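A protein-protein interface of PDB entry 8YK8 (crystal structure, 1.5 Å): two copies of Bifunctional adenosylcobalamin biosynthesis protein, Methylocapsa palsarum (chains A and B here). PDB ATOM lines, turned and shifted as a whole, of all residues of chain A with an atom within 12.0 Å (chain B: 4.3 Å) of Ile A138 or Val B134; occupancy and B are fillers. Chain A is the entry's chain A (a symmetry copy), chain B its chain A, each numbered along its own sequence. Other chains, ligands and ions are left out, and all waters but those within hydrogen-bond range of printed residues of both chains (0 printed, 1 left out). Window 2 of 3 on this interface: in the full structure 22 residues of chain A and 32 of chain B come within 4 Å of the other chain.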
ATOM      1  N   GLU A 133     -14.807  -7.807 -33.056  1.00  0.00           N
ATOM      2  CA  GLU A 133     -15.130  -9.121 -32.504  1.00  0.00           C
ATOM      3  C   GLU A 133     -14.141  -9.424 -31.392  1.00  0.00           C
ATOM      4  O   GLU A 133     -12.918  -9.401 -31.634  1.00  0.00           O
ATOM      5  CB  GLU A 133     -15.054 -10.195 -33.593  1.00  0.00           C
ATOM      6  CG  GLU A 133     -15.311 -11.575 -33.043  1.00  0.00           C
ATOM      7  CD  GLU A 133     -16.691 -11.755 -32.491  1.00  0.00           C
ATOM      8  OE1 GLU A 133     -16.902 -12.194 -31.320  1.00  0.00           O
ATOM      9  OE2 GLU A 133     -17.641 -11.500 -33.330  1.00  0.00           O
ATOM     10  N   VAL A 134     -14.677  -9.705 -30.189  1.00  0.00           N
ATOM     11  CA  VAL A 134     -13.789 -10.079 -29.076  1.00  0.00           C
ATOM     12  C   VAL A 134     -14.140 -11.412 -28.471  1.00  0.00           C
ATOM     13  O   VAL A 134     -13.595 -11.735 -27.422  1.00  0.00           O
ATOM     14  CB  VAL A 134     -13.748  -8.977 -28.010  1.00  0.00           C
ATOM     15  CG1 VAL A 134     -13.384  -7.634 -28.610  1.00  0.00           C
ATOM     16  CG2 VAL A 134     -15.057  -8.895 -27.254  1.00  0.00           C
ATOM     17  N   GLY A 135     -15.082 -12.146 -29.032  1.00  0.00           N
ATOM     18  CA  GLY A 135     -15.708 -13.283 -28.373  1.00  0.00           C
ATOM     19  C   GLY A 135     -15.158 -14.612 -28.811  1.00  0.00           C
ATOM     20  O   GLY A 135     -15.688 -15.632 -28.293  1.00  0.00           O
ATOM     21  N   ALA A 136     -14.156 -14.691 -29.686  1.00  0.00           N
ATOM     22  CA  ALA A 136     -13.805 -15.998 -30.290  1.00  0.00           C
ATOM     23  C   ALA A 136     -12.463 -16.518 -29.791  1.00  0.00           C
ATOM     24  O   ALA A 136     -11.872 -17.406 -30.407  1.00  0.00           O
ATOM     25  CB  ALA A 136     -13.796 -15.825 -31.776  1.00  0.00           C
ATOM     26  N   GLY A 137     -12.097 -16.086 -28.591  1.00  0.00           N
ATOM     27  CA  GLY A 137     -11.033 -16.700 -27.820  1.00  0.00           C
ATOM     28  C   GLY A 137     -11.543 -17.405 -26.607  1.00  0.00           C
ATOM     29  O   GLY A 137     -12.736 -17.685 -26.448  1.00  0.00           O
ATOM     30  N   ILE A 138     -10.618 -17.649 -25.661  1.00  0.00           N
ATOM     31  CA  ILE A 138     -10.980 -18.401 -24.427  1.00  0.00           C
ATOM     32  C   ILE A 138     -11.674 -17.499 -23.398  1.00  0.00           C
ATOM     33  O   ILE A 138     -11.587 -16.297 -23.479  1.00  0.00           O
ATOM     34  CB  ILE A 138      -9.699 -19.066 -23.892  1.00  0.00           C
ATOM     35  CG1 ILE A 138      -8.740 -18.040 -23.285  1.00  0.00           C
ATOM     36  CG2 ILE A 138      -9.050 -19.921 -24.969  1.00  0.00           C
ATOM     37  CD1 ILE A 138      -7.681 -18.666 -22.400  1.00  0.00           C
ATOM     38  N   VAL A 139     -12.296 -18.106 -22.402  1.00  0.00           N
ATOM     39  CA  VAL A 139     -12.948 -17.312 -21.326  1.00  0.00           C
ATOM     40  C   VAL A 139     -11.870 -16.553 -20.564  1.00  0.00           C
ATOM     41  O   VAL A 139     -10.915 -17.171 -20.100  1.00  0.00           O
ATOM     42  CB  VAL A 139     -13.758 -18.192 -20.359  1.00  0.00           C
ATOM     43  CG1 VAL A 139     -14.475 -17.354 -19.333  1.00  0.00           C
ATOM     44  CG2 VAL A 139     -14.755 -19.077 -21.059  1.00  0.00           C
ATOM     45  N   PRO A 140     -12.017 -15.215 -20.423  1.00  0.00           N
ATOM     46  CA  PRO A 140     -11.113 -14.379 -19.641  1.00  0.00           C
ATOM     47  C   PRO A 140     -11.068 -14.862 -18.184  1.00  0.00           C
ATOM     48  O   PRO A 140     -12.007 -15.387 -17.684  1.00  0.00           O
ATOM     49  CB  PRO A 140     -11.658 -12.957 -19.770  1.00  0.00           C
ATOM     50  CG  PRO A 140     -12.416 -12.997 -21.087  1.00  0.00           C
ATOM     51  CD  PRO A 140     -12.992 -14.395 -21.163  1.00  0.00           C
ATOM     52  N   ASP A 141      -9.904 -14.647 -17.570  1.00  0.00           N
ATOM     53  CA  ASP A 141      -9.636 -15.124 -16.196  1.00  0.00           C
ATOM     54  C   ASP A 141     -10.125 -14.115 -15.153  1.00  0.00           C
ATOM     55  O   ASP A 141      -9.816 -14.315 -13.970  1.00  0.00           O
ATOM     56  CB  ASP A 141      -8.145 -15.409 -16.010  1.00  0.00           C
ATOM     57  CG  ASP A 141      -7.196 -14.223 -16.145  1.00  0.00           C
ATOM     58  OD1 ASP A 141      -7.630 -13.066 -16.056  1.00  0.00           O
ATOM     59  OD2 ASP A 141      -5.979 -14.463 -16.312  1.00  0.00           O
ATOM     60  N   ASN A 142     -10.840 -13.066 -15.545  1.00  0.00           N
ATOM     61  CA  ASN A 142     -11.272 -11.995 -14.614  1.00  0.00           C
ATOM     62  C   ASN A 142     -12.617 -11.438 -15.058  1.00  0.00           C
ATOM     63  O   ASN A 142     -12.960 -11.433 -16.277  1.00  0.00           O
ATOM     64  CB  ASN A 142     -10.217 -10.913 -14.419  1.00  0.00           C
ATOM     65  CG  ASN A 142     -10.082 -10.002 -15.623  1.00  0.00           C
ATOM     66  OD1 ASN A 142     -10.836  -9.039 -15.737  1.00  0.00           O
ATOM     67  ND2 ASN A 142      -9.168 -10.354 -16.510  1.00  0.00           N
ATOM     68  N   ALA A 143     -13.378 -10.946 -14.104  1.00  0.00           N
ATOM     69  CA  ALA A 143     -14.800 -10.605 -14.297  1.00  0.00           C
ATOM     70  C   ALA A 143     -14.943  -9.350 -15.170  1.00  0.00           C
ATOM     71  O   ALA A 143     -15.949  -9.259 -15.905  1.00  0.00           O
ATOM     72  CB  ALA A 143     -15.452 -10.482 -12.929  1.00  0.00           C
ATOM     73  N   LEU A 144     -14.013  -8.436 -15.111  1.00  0.00           N
ATOM     74  CA  LEU A 144     -14.051  -7.183 -15.890  1.00  0.00           C
ATOM     75  C   LEU A 144     -13.946  -7.588 -17.366  1.00  0.00           C
ATOM     76  O   LEU A 144     -14.759  -7.100 -18.186  1.00  0.00           O
ATOM     77  CB  LEU A 144     -12.875  -6.312 -15.454  1.00  0.00           C
ATOM     78  CG  LEU A 144     -12.994  -4.834 -15.728  1.00  0.00           C
ATOM     79  CD1 LEU A 144     -14.297  -4.251 -15.184  1.00  0.00           C
ATOM     80  CD2 LEU A 144     -11.805  -4.123 -15.121  1.00  0.00           C
ATOM     81  N   ALA A 145     -12.989  -8.442 -17.679  1.00  0.00           N
ATOM     82  CA  ALA A 145     -12.774  -8.848 -19.086  1.00  0.00           C
ATOM     83  C   ALA A 145     -13.964  -9.705 -19.520  1.00  0.00           C
ATOM     84  O   ALA A 145     -14.437  -9.618 -20.703  1.00  0.00           O
ATOM     85  CB  ALA A 145     -11.469  -9.561 -19.240  1.00  0.00           C
ATOM     86  N   ARG A 146     -14.510 -10.545 -18.646  1.00  0.00           N
ATOM     87  CA  ARG A 146     -15.671 -11.368 -19.039  1.00  0.00           C
ATOM     88  C   ARG A 146     -16.851 -10.458 -19.332  1.00  0.00           C
ATOM     89  O   ARG A 146     -17.623 -10.725 -20.286  1.00  0.00           O
ATOM     90  CB  ARG A 146     -16.060 -12.410 -17.974  1.00  0.00           C
ATOM     91  CG  ARG A 146     -15.104 -13.591 -17.862  1.00  0.00           C
ATOM     92  CD  ARG A 146     -15.814 -14.831 -17.270  1.00  0.00           C
ATOM     93  NE  ARG A 146     -16.142 -14.604 -15.871  1.00  0.00           N
ATOM     94  CZ  ARG A 146     -15.246 -14.597 -14.886  1.00  0.00           C
ATOM     95  NH1 ARG A 146     -13.959 -14.789 -15.137  1.00  0.00           N
ATOM     96  NH2 ARG A 146     -15.630 -14.404 -13.631  1.00  0.00           N
ATOM     97  N   ALA A 147     -17.082  -9.431 -18.517  1.00  0.00           N
ATOM     98  CA  ALA A 147     -18.212  -8.521 -18.697  1.00  0.00           C
ATOM     99  C   ALA A 147     -18.028  -7.780 -20.010  1.00  0.00           C
ATOM    100  O   ALA A 147     -19.019  -7.508 -20.697  1.00  0.00           O
ATOM    101  CB  ALA A 147     -18.314  -7.560 -17.532  1.00  0.00           C
ATOM    102  N   PHE A 148     -16.812  -7.364 -20.247  1.00  0.00           N
ATOM    103  CA  PHE A 148     -16.541  -6.579 -21.464  1.00  0.00           C
ATOM    104  C   PHE A 148     -16.832  -7.461 -22.680  1.00  0.00           C
ATOM    105  O   PHE A 148     -17.478  -6.991 -23.685  1.00  0.00           O
ATOM    106  CB  PHE A 148     -15.106  -6.084 -21.499  1.00  0.00           C
ATOM    107  CG  PHE A 148     -14.844  -5.316 -22.769  1.00  0.00           C
ATOM    108  CD1 PHE A 148     -15.277  -4.020 -22.880  1.00  0.00           C
ATOM    109  CD2 PHE A 148     -14.236  -5.927 -23.839  1.00  0.00           C
ATOM    110  CE1 PHE A 148     -15.061  -3.306 -24.043  1.00  0.00           C
ATOM    111  CE2 PHE A 148     -14.015  -5.210 -25.004  1.00  0.00           C
ATOM    112  CZ  PHE A 148     -14.414  -3.899 -25.080  1.00  0.00           C
ATOM    113  N   ARG A 149     -16.303  -8.663 -22.683  1.00  0.00           N
ATOM    114  CA  ARG A 149     -16.528  -9.627 -23.780  1.00  0.00           C
ATOM    115  C   ARG A 149     -18.030  -9.813 -24.013  1.00  0.00           C
ATOM    116  O   ARG A 149     -18.545  -9.796 -25.171  1.00  0.00           O
ATOM    117  CB  ARG A 149     -15.777 -10.906 -23.405  1.00  0.00           C
ATOM    118  CG  ARG A 149     -15.825 -12.009 -24.426  1.00  0.00           C
ATOM    119  CD  ARG A 149     -14.784 -12.918 -23.828  1.00  0.00           C
ATOM    120  NE  ARG A 149     -14.596 -14.171 -24.474  1.00  0.00           N
ATOM    121  CZ  ARG A 149     -15.080 -15.331 -24.091  1.00  0.00           C
ATOM    122  NH1 ARG A 149     -14.726 -16.346 -24.816  1.00  0.00           N
ATOM    123  NH2 ARG A 149     -15.955 -15.510 -23.096  1.00  0.00           N
ATOM    124  N   ASP A 150     -18.829 -10.031 -22.957  1.00  0.00           N
ATOM    125  CA  ASP A 150     -20.269 -10.219 -23.059  1.00  0.00           C
ATOM    126  C   ASP A 150     -20.894  -8.952 -23.653  1.00  0.00           C
ATOM    127  O   ASP A 150     -21.734  -9.033 -24.536  1.00  0.00           O
ATOM    128  CB  ASP A 150     -20.866 -10.504 -21.666  1.00  0.00           C
ATOM    129  CG  ASP A 150     -22.251 -11.096 -21.747  1.00  0.00           C
ATOM    130  OD1 ASP A 150     -23.196 -10.325 -21.836  1.00  0.00           O
ATOM    131  OD2 ASP A 150     -22.364 -12.341 -21.789  1.00  0.00           O
ATOM    132  N   ASN B 132     -18.945 -23.049 -28.926  1.00  0.00           N
ATOM    133  CA  ASN B 132     -18.142 -21.831 -29.105  1.00  0.00           C
ATOM    134  C   ASN B 132     -16.962 -22.055 -30.020  1.00  0.00           C
ATOM    135  O   ASN B 132     -16.308 -23.110 -30.005  1.00  0.00           O
ATOM    136  CB  ASN B 132     -17.528 -21.375 -27.780  1.00  0.00           C
ATOM    137  CG  ASN B 132     -18.578 -20.731 -26.926  1.00  0.00           C
ATOM    138  OD1 ASN B 132     -19.518 -21.362 -26.460  1.00  0.00           O
ATOM    139  ND2 ASN B 132     -18.381 -19.489 -26.589  1.00  0.00           N
ATOM    140  N   GLU B 133     -16.637 -21.027 -30.794  1.00  0.00           N
ATOM    141  CA  GLU B 133     -15.292 -20.823 -31.330  1.00  0.00           C
ATOM    142  C   GLU B 133     -14.429 -20.231 -30.229  1.00  0.00           C
ATOM    143  O   GLU B 133     -14.782 -19.174 -29.671  1.00  0.00           O
ATOM    144  CB  GLU B 133     -15.333 -19.882 -32.539  1.00  0.00           C
ATOM    145  CG  GLU B 133     -13.954 -19.591 -33.073  1.00  0.00           C
ATOM    146  CD  GLU B 133     -13.248 -20.798 -33.610  1.00  0.00           C
ATOM    147  OE1 GLU B 133     -12.086 -21.131 -33.229  1.00  0.00           O
ATOM    148  OE2 GLU B 133     -13.892 -21.423 -34.543  1.00  0.00           O
ATOM    149  N   VAL B 134     -13.307 -20.915 -29.930  1.00  0.00           N
ATOM    150  CA  VAL B 134     -12.380 -20.371 -28.924  1.00  0.00           C
ATOM    151  C   VAL B 134     -10.982 -20.196 -29.453  1.00  0.00           C
ATOM    152  O   VAL B 134     -10.088 -19.934 -28.656  1.00  0.00           O
ATOM    153  CB  VAL B 134     -12.392 -21.221 -27.648  1.00  0.00           C
ATOM    154  CG1 VAL B 134     -13.796 -21.392 -27.104  1.00  0.00           C
ATOM    155  CG2 VAL B 134     -11.734 -22.565 -27.879  1.00  0.00           C
ATOM    156  N   GLY B 135     -10.743 -20.418 -30.731  1.00  0.00           N
ATOM    157  CA  GLY B 135      -9.405 -20.580 -31.280  1.00  0.00           C
ATOM    158  C   GLY B 135      -8.872 -19.342 -31.945  1.00  0.00           C
ATOM    159  O   GLY B 135      -7.727 -19.438 -32.464  1.00  0.00           O
ATOM    160  N   ALA B 136      -9.574 -18.209 -31.963  1.00  0.00           N
ATOM    161  CA  ALA B 136      -9.147 -17.089 -32.836  1.00  0.00           C
ATOM    162  C   ALA B 136      -8.617 -15.909 -32.032  1.00  0.00           C
ATOM    163  O   ALA B 136      -8.520 -14.797 -32.552  1.00  0.00           O
ATOM    164  CB  ALA B 136     -10.323 -16.689 -33.669  1.00  0.00           C
ATOM    165  N   PRO B 140      -2.932 -19.205 -25.215  1.00  0.00           N
ATOM    166  CA  PRO B 140      -3.078 -19.135 -23.766  1.00  0.00           C
ATOM    167  C   PRO B 140      -1.717 -19.331 -23.083  1.00  0.00           C
ATOM    168  O   PRO B 140      -0.872 -19.995 -23.584  1.00  0.00           O
ATOM    169  CB  PRO B 140      -4.079 -20.233 -23.403  1.00  0.00           C
ATOM    170  CG  PRO B 140      -4.883 -20.402 -24.682  1.00  0.00           C
ATOM    171  CD  PRO B 140      -3.891 -20.159 -25.800  1.00  0.00           C
ATOM    172  N   ALA B 145      -5.535 -24.198 -20.457  1.00  0.00           N
ATOM    173  CA  ALA B 145      -6.283 -23.372 -21.431  1.00  0.00           C
ATOM    174  C   ALA B 145      -5.835 -23.775 -22.837  1.00  0.00           C
ATOM    175  O   ALA B 145      -6.671 -23.820 -23.802  1.00  0.00           O
ATOM    176  CB  ALA B 145      -6.078 -21.915 -21.161  1.00  0.00           C
ATOM    177  N   ARG B 149      -8.482 -25.161 -25.601  1.00  0.00           N
ATOM    178  CA  ARG B 149      -8.562 -24.517 -26.929  1.00  0.00           C
ATOM    179  C   ARG B 149      -8.394 -25.567 -28.031  1.00  0.00           C
ATOM    180  O   ARG B 149      -9.157 -25.619 -29.041  1.00  0.00           O
ATOM    181  CB  ARG B 149      -7.514 -23.403 -26.944  1.00  0.00           C
ATOM    182  CG  ARG B 149      -7.469 -22.571 -28.196  1.00  0.00           C
ATOM    183  CD  ARG B 149      -6.559 -21.475 -27.709  1.00  0.00           C
ATOM    184  NE  ARG B 149      -6.176 -20.501 -28.672  1.00  0.00           N
ATOM    185  CZ  ARG B 149      -5.037 -20.447 -29.323  1.00  0.00           C
ATOM    186  NH1 ARG B 149      -4.898 -19.428 -30.115  1.00  0.00           N
ATOM    187  NH2 ARG B 149      -4.087 -21.389 -29.294  1.00  0.00           N
ATOM    188  N   GLN B 152     -11.448 -28.086 -28.083  1.00  0.00           N
ATOM    189  CA  GLN B 152     -12.687 -27.457 -28.595  1.00  0.00           C
ATOM    190  C   GLN B 152     -12.585 -27.291 -30.108  1.00  0.00           C
ATOM    191  O   GLN B 152     -13.554 -27.557 -30.818  1.00  0.00           O
ATOM    192  CB  GLN B 152     -12.913 -26.102 -27.944  1.00  0.00           C
ATOM    193  CG  GLN B 152     -14.151 -25.368 -28.472  1.00  0.00           C
ATOM    194  CD  GLN B 152     -15.437 -26.061 -28.144  1.00  0.00           C
ATOM    195  OE1 GLN B 152     -15.955 -25.884 -27.040  1.00  0.00           O
ATOM    196  NE2 GLN B 152     -15.905 -26.917 -29.024  1.00  0.00           N
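The backbone carbonyl oxygen (O) of Glu B133 lies close to the backbone carbonyl oxygen (O) of Ala A136 (3.5 Å). O of Ala A136 lies within hydrogen-bond range of N of Ala B136, 2.9 Å away. The backbone carbonyl oxygen (O) of Ala A136 lies within hydrogen-bond range of the backbone NH (N) of Gly B135 (3.2 Å).
Hydrophobic or aromatic side chains of chain A that line the printed part of chain B: Ala A136 and Ile A138. Of the 9 printed residues of chain B, 5 touch a printed residue of chain A. Along chain B the printed residues that touch a printed residue of chain A span positions 133 to 145.
Among the printed residues, merely in contact across the chains: Ala A136 with Val B134 (3.1 Å), Gly A137 with Val B134 (3.5 Å), Ile A138 with Val B134 (3.8 Å), Ile A138 with Ala B145 (3.8 Å) and Gly A135 with Glu B133 (3.9 Å).
Ala A136 touches Glu B133, but with the chains exchanged Glu A133 does not touch Ala B136 (7.0 Å). Ala A136 touches Val B134, but with the chains exchanged Val A134 does not touch Ala B136 (7.7 Å). Ala A136 touches Gly B135, but with the chains exchanged Gly A135 does not touch Ala B136 (7.2 Å). Ala B136 touches its own counterpart, Ala A136. Positions printed for both chains: 133, 134, 135, 136, 140, 145 and 149. Of the 8 pairs that touch across the chains among the printed residues, 1 has its exchanged pair printed and touching as well.
OE1 of Glu A133 is in hydrogen-bond range of N of Gly A135 (2.9 Å). O of Gly A137 is in hydrogen-bond range of NH1 of Arg A149 (2.9 Å). OE1 of Glu B133 sits at hydrogen-bond distance from N of Gly B135 (2.9 Å). The backbone carbonyl oxygen of Ile A138 sits at hydrogen-bond distance from the guanidinium group of Arg A149 (3.4 Å).
Of the printed residues of chain B, Ala A136 touches Glu B133 (3.4 Å), Val B134 (3.1 Å), Gly B135 (3.2 Å) and Ala B136 (2.9 Å). Of the printed residues of chain B, Gly A137 touches Val B134 (3.5 Å). Leu A144 touches none of the printed residues of chain B. No residue of chain A comes within 4 Å of Asn B132. Glu B133 touches just these residues of chain A: Gly A135 (3.9 Å) and Ala A136 (3.4 Å). Of the printed residues of chain A, Val B134 touches Ala A136 (3.1 Å), Gly A137 (3.5 Å) and Ile A138 (3.8 Å). Gly B135 touches just one residue of chain A: Ala A136 (3.2 Å). Ala B136 touches just one residue of chain A: Ala A136. Of the printed residues of chain A, Ala B145 touches Ile A138 (3.8 Å). No residue of chain A comes within 4 Å of Gln B152. The nearest residue of chain A that does not touch Val B134 is Arg A149 (5.6 Å).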
